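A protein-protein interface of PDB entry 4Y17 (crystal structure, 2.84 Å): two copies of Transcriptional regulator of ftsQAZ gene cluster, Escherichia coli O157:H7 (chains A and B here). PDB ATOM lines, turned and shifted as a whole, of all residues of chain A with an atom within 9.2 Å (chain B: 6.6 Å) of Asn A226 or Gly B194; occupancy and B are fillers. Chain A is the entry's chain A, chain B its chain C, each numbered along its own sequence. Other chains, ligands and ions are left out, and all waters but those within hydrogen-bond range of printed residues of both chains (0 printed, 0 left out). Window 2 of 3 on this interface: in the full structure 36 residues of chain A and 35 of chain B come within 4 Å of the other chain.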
ATOM      1  N   PHE A  52     -12.645  25.866  26.755  1.00  0.00           N
ATOM      2  CA  PHE A  52     -13.049  27.218  27.127  1.00  0.00           C
ATOM      3  C   PHE A  52     -13.610  28.032  25.963  1.00  0.00           C
ATOM      4  O   PHE A  52     -14.445  28.913  26.165  1.00  0.00           O
ATOM      5  CB  PHE A  52     -11.860  27.956  27.743  1.00  0.00           C
ATOM      6  CG  PHE A  52     -11.293  27.282  28.961  1.00  0.00           C
ATOM      7  CD1 PHE A  52     -11.875  27.465  30.204  1.00  0.00           C
ATOM      8  CD2 PHE A  52     -10.177  26.467  28.864  1.00  0.00           C
ATOM      9  CE1 PHE A  52     -11.357  26.851  31.328  1.00  0.00           C
ATOM     10  CE2 PHE A  52      -9.654  25.846  29.986  1.00  0.00           C
ATOM     11  CZ  PHE A  52     -10.246  26.041  31.220  1.00  0.00           C
ATOM     12  N   THR A  53     -13.153  27.734  24.751  1.00  0.00           N
ATOM     13  CA  THR A  53     -13.536  28.507  23.568  1.00  0.00           C
ATOM     14  C   THR A  53     -14.744  27.899  22.854  1.00  0.00           C
ATOM     15  O   THR A  53     -15.532  28.619  22.240  1.00  0.00           O
ATOM     16  CB  THR A  53     -12.366  28.634  22.579  1.00  0.00           C
ATOM     17  OG1 THR A  53     -11.851  27.335  22.267  1.00  0.00           O
ATOM     18  CG2 THR A  53     -11.255  29.479  23.185  1.00  0.00           C
ATOM     19  N   LEU A 188      -0.317  18.066  39.054  1.00  0.00           N
ATOM     20  CA  LEU A 188      -1.204  19.049  38.447  1.00  0.00           C
ATOM     21  C   LEU A 188      -1.411  20.237  39.382  1.00  0.00           C
ATOM     22  O   LEU A 188      -1.348  21.390  38.957  1.00  0.00           O
ATOM     23  CB  LEU A 188      -2.546  18.403  38.100  1.00  0.00           C
ATOM     24  CG  LEU A 188      -2.615  17.623  36.783  1.00  0.00           C
ATOM     25  CD1 LEU A 188      -3.998  17.016  36.609  1.00  0.00           C
ATOM     26  CD2 LEU A 188      -2.262  18.482  35.578  1.00  0.00           C
ATOM     27  N   THR A 191       1.698  22.226  39.288  1.00  0.00           N
ATOM     28  CA  THR A 191       1.797  22.865  37.984  1.00  0.00           C
ATOM     29  C   THR A 191       0.857  24.064  37.958  1.00  0.00           C
ATOM     30  O   THR A 191       1.174  25.110  37.390  1.00  0.00           O
ATOM     31  CB  THR A 191       1.444  21.893  36.838  1.00  0.00           C
ATOM     32  OG1 THR A 191       2.348  20.781  36.850  1.00  0.00           O
ATOM     33  CG2 THR A 191       1.523  22.591  35.482  1.00  0.00           C
ATOM     34  N   GLN A 215       3.880  14.241  33.087  1.00  0.00           N
ATOM     35  CA  GLN A 215       3.338  15.419  32.444  1.00  0.00           C
ATOM     36  C   GLN A 215       2.904  15.058  31.025  1.00  0.00           C
ATOM     37  O   GLN A 215       1.824  15.439  30.581  1.00  0.00           O
ATOM     38  CB  GLN A 215       4.369  16.548  32.426  1.00  0.00           C
ATOM     39  CG  GLN A 215       3.744  17.925  32.432  1.00  0.00           C
ATOM     40  CD  GLN A 215       2.961  18.173  33.714  1.00  0.00           C
ATOM     41  OE1 GLN A 215       3.545  18.371  34.780  1.00  0.00           O
ATOM     42  NE2 GLN A 215       1.638  18.122  33.623  1.00  0.00           N
ATOM     43  N   LYS A 216       3.758  14.321  30.321  1.00  0.00           N
ATOM     44  CA  LYS A 216       3.467  13.901  28.953  1.00  0.00           C
ATOM     45  C   LYS A 216       2.399  12.813  28.896  1.00  0.00           C
ATOM     46  O   LYS A 216       1.600  12.775  27.963  1.00  0.00           O
ATOM     47  CB  LYS A 216       4.738  13.398  28.262  1.00  0.00           C
ATOM     48  CG  LYS A 216       5.714  14.490  27.848  1.00  0.00           C
ATOM     49  CD  LYS A 216       6.891  13.909  27.074  1.00  0.00           C
ATOM     50  CE  LYS A 216       7.815  14.995  26.546  1.00  0.00           C
ATOM     51  NZ  LYS A 216       8.955  14.427  25.772  1.00  0.00           N
ATOM     52  N   MET A 218      -0.172  12.480  30.855  1.00  0.00           N
ATOM     53  CA  MET A 218      -1.488  13.084  31.028  1.00  0.00           C
ATOM     54  C   MET A 218      -1.924  13.741  29.726  1.00  0.00           C
ATOM     55  O   MET A 218      -3.092  13.672  29.352  1.00  0.00           O
ATOM     56  CB  MET A 218      -1.493  14.107  32.166  1.00  0.00           C
ATOM     57  CG  MET A 218      -1.431  13.489  33.555  1.00  0.00           C
ATOM     58  SD  MET A 218      -1.280  14.696  34.888  1.00  0.00           S
ATOM     59  CE  MET A 218       0.441  15.154  34.753  1.00  0.00           C
ATOM     60  N   GLN A 219      -0.972  14.367  29.040  1.00  0.00           N
ATOM     61  CA  GLN A 219      -1.230  15.014  27.757  1.00  0.00           C
ATOM     62  C   GLN A 219      -1.570  13.988  26.680  1.00  0.00           C
ATOM     63  O   GLN A 219      -2.260  14.299  25.710  1.00  0.00           O
ATOM     64  CB  GLN A 219      -0.014  15.834  27.323  1.00  0.00           C
ATOM     65  CG  GLN A 219       0.306  17.006  28.237  1.00  0.00           C
ATOM     66  CD  GLN A 219       1.681  17.624  27.988  1.00  0.00           C
ATOM     67  OE1 GLN A 219       2.151  18.434  28.786  1.00  0.00           O
ATOM     68  NE2 GLN A 219       2.333  17.239  26.891  1.00  0.00           N
ATOM     69  N   LYS A 220      -1.071  12.767  26.855  1.00  0.00           N
ATOM     70  CA  LYS A 220      -1.360  11.675  25.931  1.00  0.00           C
ATOM     71  C   LYS A 220      -2.852  11.365  25.915  1.00  0.00           C
ATOM     72  O   LYS A 220      -3.504  11.445  24.873  1.00  0.00           O
ATOM     73  CB  LYS A 220      -0.587  10.414  26.333  1.00  0.00           C
ATOM     74  CG  LYS A 220       0.869  10.357  25.898  1.00  0.00           C
ATOM     75  CD  LYS A 220       1.521   9.082  26.426  1.00  0.00           C
ATOM     76  CE  LYS A 220       3.034   9.097  26.277  1.00  0.00           C
ATOM     77  NZ  LYS A 220       3.679   8.171  27.253  1.00  0.00           N
ATOM     78  N   ILE A 222      -5.383  12.857  26.933  1.00  0.00           N
ATOM     79  CA  ILE A 222      -6.309  13.974  26.762  1.00  0.00           C
ATOM     80  C   ILE A 222      -6.106  14.571  25.379  1.00  0.00           C
ATOM     81  O   ILE A 222      -6.969  15.289  24.871  1.00  0.00           O
ATOM     82  CB  ILE A 222      -6.098  15.070  27.839  1.00  0.00           C
ATOM     83  CG1 ILE A 222      -7.207  16.131  27.758  1.00  0.00           C
ATOM     84  CG2 ILE A 222      -4.737  15.729  27.665  1.00  0.00           C
ATOM     85  CD1 ILE A 222      -7.126  17.208  28.828  1.00  0.00           C
ATOM     86  N   ASN A 223      -4.966  14.252  24.769  1.00  0.00           N
ATOM     87  CA  ASN A 223      -4.593  14.833  23.489  1.00  0.00           C
ATOM     88  C   ASN A 223      -4.494  16.339  23.677  1.00  0.00           C
ATOM     89  O   ASN A 223      -5.398  17.087  23.303  1.00  0.00           O
ATOM     90  CB  ASN A 223      -5.584  14.461  22.382  1.00  0.00           C
ATOM     91  CG  ASN A 223      -5.089  14.855  21.000  1.00  0.00           C
ATOM     92  OD1 ASN A 223      -4.208  15.702  20.858  1.00  0.00           O
ATOM     93  ND2 ASN A 223      -5.634  14.212  19.975  1.00  0.00           N
ATOM     94  N   ALA A 224      -3.382  16.771  24.261  1.00  0.00           N
ATOM     95  CA  ALA A 224      -3.161  18.177  24.554  1.00  0.00           C
ATOM     96  C   ALA A 224      -1.720  18.534  24.247  1.00  0.00           C
ATOM     97  O   ALA A 224      -0.826  17.702  24.387  1.00  0.00           O
ATOM     98  CB  ALA A 224      -3.475  18.475  26.014  1.00  0.00           C
ATOM     99  N   PRO A 225      -1.492  19.781  23.815  1.00  0.00           N
ATOM    100  CA  PRO A 225      -0.156  20.180  23.365  1.00  0.00           C
ATOM    101  C   PRO A 225       0.841  20.301  24.513  1.00  0.00           C
ATOM    102  O   PRO A 225       1.946  19.762  24.431  1.00  0.00           O
ATOM    103  CB  PRO A 225      -0.415  21.545  22.715  1.00  0.00           C
ATOM    104  CG  PRO A 225      -1.607  22.080  23.450  1.00  0.00           C
ATOM    105  CD  PRO A 225      -2.468  20.881  23.699  1.00  0.00           C
ATOM    106  N   ASN A 226       0.440  21.005  25.565  1.00  0.00           N
ATOM    107  CA  ASN A 226       1.326  21.333  26.675  1.00  0.00           C
ATOM    108  C   ASN A 226       0.723  21.026  28.044  1.00  0.00           C
ATOM    109  O   ASN A 226      -0.441  20.635  28.153  1.00  0.00           O
ATOM    110  CB  ASN A 226       1.729  22.800  26.592  1.00  0.00           C
ATOM    111  CG  ASN A 226       0.561  23.702  26.298  1.00  0.00           C
ATOM    112  OD1 ASN A 226      -0.350  23.844  27.109  1.00  0.00           O
ATOM    113  ND2 ASN A 226       0.572  24.308  25.119  1.00  0.00           N
ATOM    114  N   LYS A 227       1.533  21.205  29.082  1.00  0.00           N
ATOM    115  CA  LYS A 227       1.081  21.039  30.460  1.00  0.00           C
ATOM    116  C   LYS A 227       0.110  22.139  30.894  1.00  0.00           C
ATOM    117  O   LYS A 227      -0.575  21.997  31.906  1.00  0.00           O
ATOM    118  CB  LYS A 227       2.281  20.994  31.420  1.00  0.00           C
ATOM    119  CG  LYS A 227       3.165  22.237  31.424  1.00  0.00           C
ATOM    120  CD  LYS A 227       4.339  22.063  32.387  1.00  0.00           C
ATOM    121  CE  LYS A 227       5.007  23.389  32.730  1.00  0.00           C
ATOM    122  NZ  LYS A 227       5.923  23.265  33.902  1.00  0.00           N
ATOM    123  N   THR A 228       0.042  23.227  30.133  1.00  0.00           N
ATOM    124  CA  THR A 228      -0.798  24.360  30.515  1.00  0.00           C
ATOM    125  C   THR A 228      -2.273  24.004  30.348  1.00  0.00           C
ATOM    126  O   THR A 228      -3.091  24.309  31.216  1.00  0.00           O
ATOM    127  CB  THR A 228      -0.479  25.617  29.680  1.00  0.00           C
ATOM    128  OG1 THR A 228       0.938  25.834  29.654  1.00  0.00           O
ATOM    129  CG2 THR A 228      -1.171  26.842  30.260  1.00  0.00           C
ATOM    130  N   GLN A 229      -2.613  23.367  29.232  1.00  0.00           N
ATOM    131  CA  GLN A 229      -3.999  22.999  28.968  1.00  0.00           C
ATOM    132  C   GLN A 229      -4.498  21.934  29.936  1.00  0.00           C
ATOM    133  O   GLN A 229      -5.642  21.979  30.382  1.00  0.00           O
ATOM    134  CB  GLN A 229      -4.160  22.496  27.530  1.00  0.00           C
ATOM    135  CG  GLN A 229      -5.608  22.210  27.145  1.00  0.00           C
ATOM    136  CD  GLN A 229      -5.744  21.567  25.779  1.00  0.00           C
ATOM    137  OE1 GLN A 229      -5.960  20.360  25.666  1.00  0.00           O
ATOM    138  NE2 GLN A 229      -5.631  22.375  24.732  1.00  0.00           N
ATOM    139  N   VAL A 230      -3.635  20.984  30.271  1.00  0.00           N
ATOM    140  CA  VAL A 230      -4.020  19.891  31.151  1.00  0.00           C
ATOM    141  C   VAL A 230      -4.363  20.432  32.538  1.00  0.00           C
ATOM    142  O   VAL A 230      -5.346  20.016  33.153  1.00  0.00           O
ATOM    143  CB  VAL A 230      -2.903  18.832  31.257  1.00  0.00           C
ATOM    144  CG1 VAL A 230      -3.356  17.654  32.111  1.00  0.00           C
ATOM    145  CG2 VAL A 230      -2.508  18.341  29.871  1.00  0.00           C
ATOM    146  N   ALA A 231      -3.546  21.360  33.023  1.00  0.00           N
ATOM    147  CA  ALA A 231      -3.742  21.952  34.343  1.00  0.00           C
ATOM    148  C   ALA A 231      -5.007  22.810  34.421  1.00  0.00           C
ATOM    149  O   ALA A 231      -5.713  22.791  35.430  1.00  0.00           O
ATOM    150  CB  ALA A 231      -2.526  22.781  34.724  1.00  0.00           C
ATOM    151  N   CYS A 232      -5.289  23.562  33.362  1.00  0.00           N
ATOM    152  CA  CYS A 232      -6.438  24.465  33.350  1.00  0.00           C
ATOM    153  C   CYS A 232      -7.750  23.694  33.234  1.00  0.00           C
ATOM    154  O   CYS A 232      -8.749  24.053  33.856  1.00  0.00           O
ATOM    155  CB  CYS A 232      -6.315  25.471  32.206  1.00  0.00           C
ATOM    156  SG  CYS A 232      -5.067  26.741  32.495  1.00  0.00           S
ATOM    157  N   TYR A 233      -7.735  22.637  32.430  1.00  0.00           N
ATOM    158  CA  TYR A 233      -8.887  21.756  32.291  1.00  0.00           C
ATOM    159  C   TYR A 233      -9.196  21.088  33.625  1.00  0.00           C
ATOM    160  O   TYR A 233     -10.353  20.973  34.020  1.00  0.00           O
ATOM    161  CB  TYR A 233      -8.614  20.700  31.222  1.00  0.00           C
ATOM    162  CG  TYR A 233      -8.925  21.152  29.815  1.00  0.00           C
ATOM    163  CD1 TYR A 233      -8.382  22.324  29.311  1.00  0.00           C
ATOM    164  CD2 TYR A 233      -9.721  20.386  28.976  1.00  0.00           C
ATOM    165  CE1 TYR A 233      -8.650  22.741  28.028  1.00  0.00           C
ATOM    166  CE2 TYR A 233      -9.990  20.792  27.684  1.00  0.00           C
ATOM    167  CZ  TYR A 233      -9.447  21.969  27.216  1.00  0.00           C
ATOM    168  OH  TYR A 233      -9.702  22.386  25.934  1.00  0.00           O
ATOM    169  N   LEU B 188      -6.379  34.628  27.756  1.00  0.00           N
ATOM    170  CA  LEU B 188      -6.291  33.605  28.794  1.00  0.00           C
ATOM    171  C   LEU B 188      -7.044  32.361  28.353  1.00  0.00           C
ATOM    172  O   LEU B 188      -6.575  31.243  28.564  1.00  0.00           O
ATOM    173  CB  LEU B 188      -6.853  34.097  30.131  1.00  0.00           C
ATOM    174  CG  LEU B 188      -5.934  34.879  31.071  1.00  0.00           C
ATOM    175  CD1 LEU B 188      -6.694  35.295  32.320  1.00  0.00           C
ATOM    176  CD2 LEU B 188      -4.701  34.065  31.454  1.00  0.00           C
ATOM    177  N   ARG B 189      -8.221  32.556  27.759  1.00  0.00           N
ATOM    178  CA  ARG B 189      -9.006  31.435  27.254  1.00  0.00           C
ATOM    179  C   ARG B 189      -8.152  30.637  26.288  1.00  0.00           C
ATOM    180  O   ARG B 189      -8.212  29.410  26.248  1.00  0.00           O
ATOM    181  CB  ARG B 189     -10.280  31.897  26.538  1.00  0.00           C
ATOM    182  CG  ARG B 189     -11.386  32.363  27.457  1.00  0.00           C
ATOM    183  CD  ARG B 189     -12.700  32.558  26.715  1.00  0.00           C
ATOM    184  NE  ARG B 189     -12.704  33.712  25.821  1.00  0.00           N
ATOM    185  CZ  ARG B 189     -13.082  34.943  26.158  1.00  0.00           C
ATOM    186  NH1 ARG B 189     -13.475  35.219  27.395  1.00  0.00           N
ATOM    187  NH2 ARG B 189     -13.050  35.908  25.250  1.00  0.00           N
ATOM    188  N   TRP B 190      -7.345  31.356  25.514  1.00  0.00           N
ATOM    189  CA  TRP B 190      -6.465  30.738  24.537  1.00  0.00           C
ATOM    190  C   TRP B 190      -5.205  30.196  25.210  1.00  0.00           C
ATOM    191  O   TRP B 190      -4.672  29.165  24.803  1.00  0.00           O
ATOM    192  CB  TRP B 190      -6.107  31.744  23.441  1.00  0.00           C
ATOM    193  CG  TRP B 190      -7.254  32.015  22.513  1.00  0.00           C
ATOM    194  CD1 TRP B 190      -7.964  33.178  22.402  1.00  0.00           C
ATOM    195  CD2 TRP B 190      -7.843  31.097  21.585  1.00  0.00           C
ATOM    196  NE1 TRP B 190      -8.950  33.042  21.456  1.00  0.00           N
ATOM    197  CE2 TRP B 190      -8.898  31.774  20.939  1.00  0.00           C
ATOM    198  CE3 TRP B 190      -7.579  29.770  21.234  1.00  0.00           C
ATOM    199  CZ2 TRP B 190      -9.685  31.168  19.961  1.00  0.00           C
ATOM    200  CZ3 TRP B 190      -8.361  29.171  20.263  1.00  0.00           C
ATOM    201  CH2 TRP B 190      -9.402  29.869  19.638  1.00  0.00           C
ATOM    202  N   THR B 191      -4.737  30.885  26.246  1.00  0.00           N
ATOM    203  CA  THR B 191      -3.604  30.398  27.026  1.00  0.00           C
ATOM    204  C   THR B 191      -3.972  29.086  27.706  1.00  0.00           C
ATOM    205  O   THR B 191      -3.157  28.166  27.790  1.00  0.00           O
ATOM    206  CB  THR B 191      -3.159  31.422  28.091  1.00  0.00           C
ATOM    207  OG1 THR B 191      -2.748  32.636  27.452  1.00  0.00           O
ATOM    208  CG2 THR B 191      -2.003  30.875  28.929  1.00  0.00           C
ATOM    209  N   ALA B 192      -5.211  29.006  28.183  1.00  0.00           N
ATOM    210  CA  ALA B 192      -5.697  27.806  28.851  1.00  0.00           C
ATOM    211  C   ALA B 192      -5.885  26.665  27.855  1.00  0.00           C
ATOM    212  O   ALA B 192      -5.963  25.503  28.246  1.00  0.00           O
ATOM    213  CB  ALA B 192      -6.997  28.098  29.577  1.00  0.00           C
ATOM    214  N   GLU B 193      -5.971  27.003  26.571  1.00  0.00           N
ATOM    215  CA  GLU B 193      -6.063  25.999  25.512  1.00  0.00           C
ATOM    216  C   GLU B 193      -4.674  25.615  25.006  1.00  0.00           C
ATOM    217  O   GLU B 193      -4.538  24.734  24.154  1.00  0.00           O
ATOM    218  CB  GLU B 193      -6.924  26.515  24.357  1.00  0.00           C
ATOM    219  CG  GLU B 193      -8.394  26.699  24.714  1.00  0.00           C
ATOM    220  CD  GLU B 193      -9.172  25.398  24.690  1.00  0.00           C
ATOM    221  OE1 GLU B 193      -9.389  24.852  23.586  1.00  0.00           O
ATOM    222  OE2 GLU B 193      -9.565  24.919  25.775  1.00  0.00           O
ATOM    223  N   GLY B 194      -3.647  26.270  25.543  1.00  0.00           N
ATOM    224  CA  GLY B 194      -2.271  25.938  25.219  1.00  0.00           C
ATOM    225  C   GLY B 194      -1.707  26.609  23.980  1.00  0.00           C
ATOM    226  O   GLY B 194      -0.835  26.046  23.319  1.00  0.00           O
ATOM    227  N   LYS B 195      -2.193  27.805  23.657  1.00  0.00           N
ATOM    228  CA  LYS B 195      -1.637  28.553  22.536  1.00  0.00           C
ATOM    229  C   LYS B 195      -0.404  29.321  22.999  1.00  0.00           C
ATOM    230  O   LYS B 195      -0.402  29.899  24.084  1.00  0.00           O
ATOM    231  CB  LYS B 195      -2.659  29.535  21.952  1.00  0.00           C
ATOM    232  CG  LYS B 195      -4.034  28.952  21.660  1.00  0.00           C
ATOM    233  CD  LYS B 195      -4.000  27.824  20.653  1.00  0.00           C
ATOM    234  CE  LYS B 195      -5.392  27.576  20.097  1.00  0.00           C
ATOM    235  NZ  LYS B 195      -5.433  26.432  19.151  1.00  0.00           N
ATOM    236  N   THR B 196       0.643  29.325  22.180  1.00  0.00           N
ATOM    237  CA  THR B 196       1.824  30.127  22.470  1.00  0.00           C
ATOM    238  C   THR B 196       1.475  31.579  22.162  1.00  0.00           C
ATOM    239  O   THR B 196       0.513  31.842  21.442  1.00  0.00           O
ATOM    240  CB  THR B 196       3.049  29.674  21.639  1.00  0.00           C
ATOM    241  OG1 THR B 196       3.248  28.265  21.801  1.00  0.00           O
ATOM    242  CG2 THR B 196       4.319  30.415  22.064  1.00  0.00           C
ATOM    243  N   GLU B 199       1.072  32.046  18.596  1.00  0.00           N
ATOM    244  CA  GLU B 199      -0.160  31.513  18.020  1.00  0.00           C
ATOM    245  C   GLU B 199      -1.355  32.422  18.302  1.00  0.00           C
ATOM    246  O   GLU B 199      -2.204  32.628  17.436  1.00  0.00           O
ATOM    247  CB  GLU B 199      -0.436  30.109  18.560  1.00  0.00           C
ATOM    248  CG  GLU B 199       0.626  29.086  18.191  1.00  0.00           C
ATOM    249  CD  GLU B 199       0.330  27.710  18.757  1.00  0.00           C
ATOM    250  OE1 GLU B 199       0.589  27.491  19.959  1.00  0.00           O
ATOM    251  OE2 GLU B 199      -0.163  26.848  18.000  1.00  0.00           O
ATOM    252  N   LYS B 227       2.246  32.199  33.039  1.00  0.00           N
ATOM    253  CA  LYS B 227       1.070  32.279  32.192  1.00  0.00           C
ATOM    254  C   LYS B 227       0.143  31.156  32.638  1.00  0.00           C
ATOM    255  O   LYS B 227      -1.064  31.180  32.400  1.00  0.00           O
ATOM    256  CB  LYS B 227       1.444  32.131  30.709  1.00  0.00           C
ATOM    257  CG  LYS B 227       2.066  30.779  30.343  1.00  0.00           C
ATOM    258  CD  LYS B 227       2.464  30.714  28.871  1.00  0.00           C
ATOM    259  CE  LYS B 227       2.652  29.276  28.398  1.00  0.00           C
ATOM    260  NZ  LYS B 227       2.727  29.182  26.913  1.00  0.00           N
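N of Phe A52 lies within hydrogen-bond range of OE2 of Glu B193 (3.4 Å). The side-chain amide nitrogen of Asn A226 lies within hydrogen-bond range of the backbone carbonyl oxygen of Gly B194 (2.9 Å). The side-chain amide nitrogen of Gln A229 lies within hydrogen-bond range of the backbone carbonyl oxygen of Glu B193 (2.7 Å). The side-chain hydroxyl of Tyr A233 is in hydrogen-bond range of the side-chain carboxylate of Glu B193.
The backbone carbonyl oxygen (O) of Asn A226 sits close to the side-chain amide oxygen (OE1) of Gln A219, 3.5 Å away. The backbone NH (N) of Thr A228 lies close to the side-chain amide oxygen (OD1) of Asn A226 (3.1 Å). N of Gln A229 is in hydrogen-bond range of OD1 of Asn A226 (3.1 Å). SG of Cys A232 sits at hydrogen-bond distance from O of Thr A228, 3.4 Å away. The backbone carbonyl oxygen (O) of Trp B190 sits at hydrogen-bond distance from the backbone NH (N) of Lys B195, at 3.1 Å.
CE2 of Phe A52 touches CB of Ala B192, at 3.5 Å. Thr A53 touches Trp B190. Thr A53 touches Glu B193. O of Thr B191 touches CG2 of Thr A228, at 3.4 Å. Gln A229 touches Ala B192. SG of Cys A232 touches CB of Ala B192, at 3.8 Å. O of Ala B192 touches CE1 of Tyr A233, at 3.9 Å.
Printed residues of chain B within 4 Å of Thr A53: Trp B190 (3.96 Å) and Glu B193 (3.7 Å). Of chain B, only Gly B194 (2.9 Å) comes within 4 Å of Asn A226. Of the printed residues of chain B, Cys A232 touches Ala B192 (3.8 Å). Of the printed residues of chain A, Thr B191 touches Thr A228. Of the printed residues of chain A, Ala B192 touches Phe A52 (3.5 Å), Gln A229 (3.3 Å), Cys A232 (3.8 Å) and Tyr A233 (3.9 Å). Gly B194 touches just one residue of chain A: Asn A226 (2.9 Å). The nearest residue of chain B that does not touch Asn A226 is Lys B195 (4.7 Å).
Of the 11 printed residues of chain B, 5 touch a printed residue of chain A. Of the 21 printed residues of chain A, 7 touch a printed residue of chain B. Hydrophobic or aromatic side chains of chain A within 4 Å of the printed part of chain B: Phe A52 and Tyr A233. Along chain A the printed residues that touch a printed residue of chain B span positions 52 to 233.
3 positions are printed for both chains. Of the 11 pairs that touch across the chains among the printed residues, none has its exchanged pair printed and touching as well.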
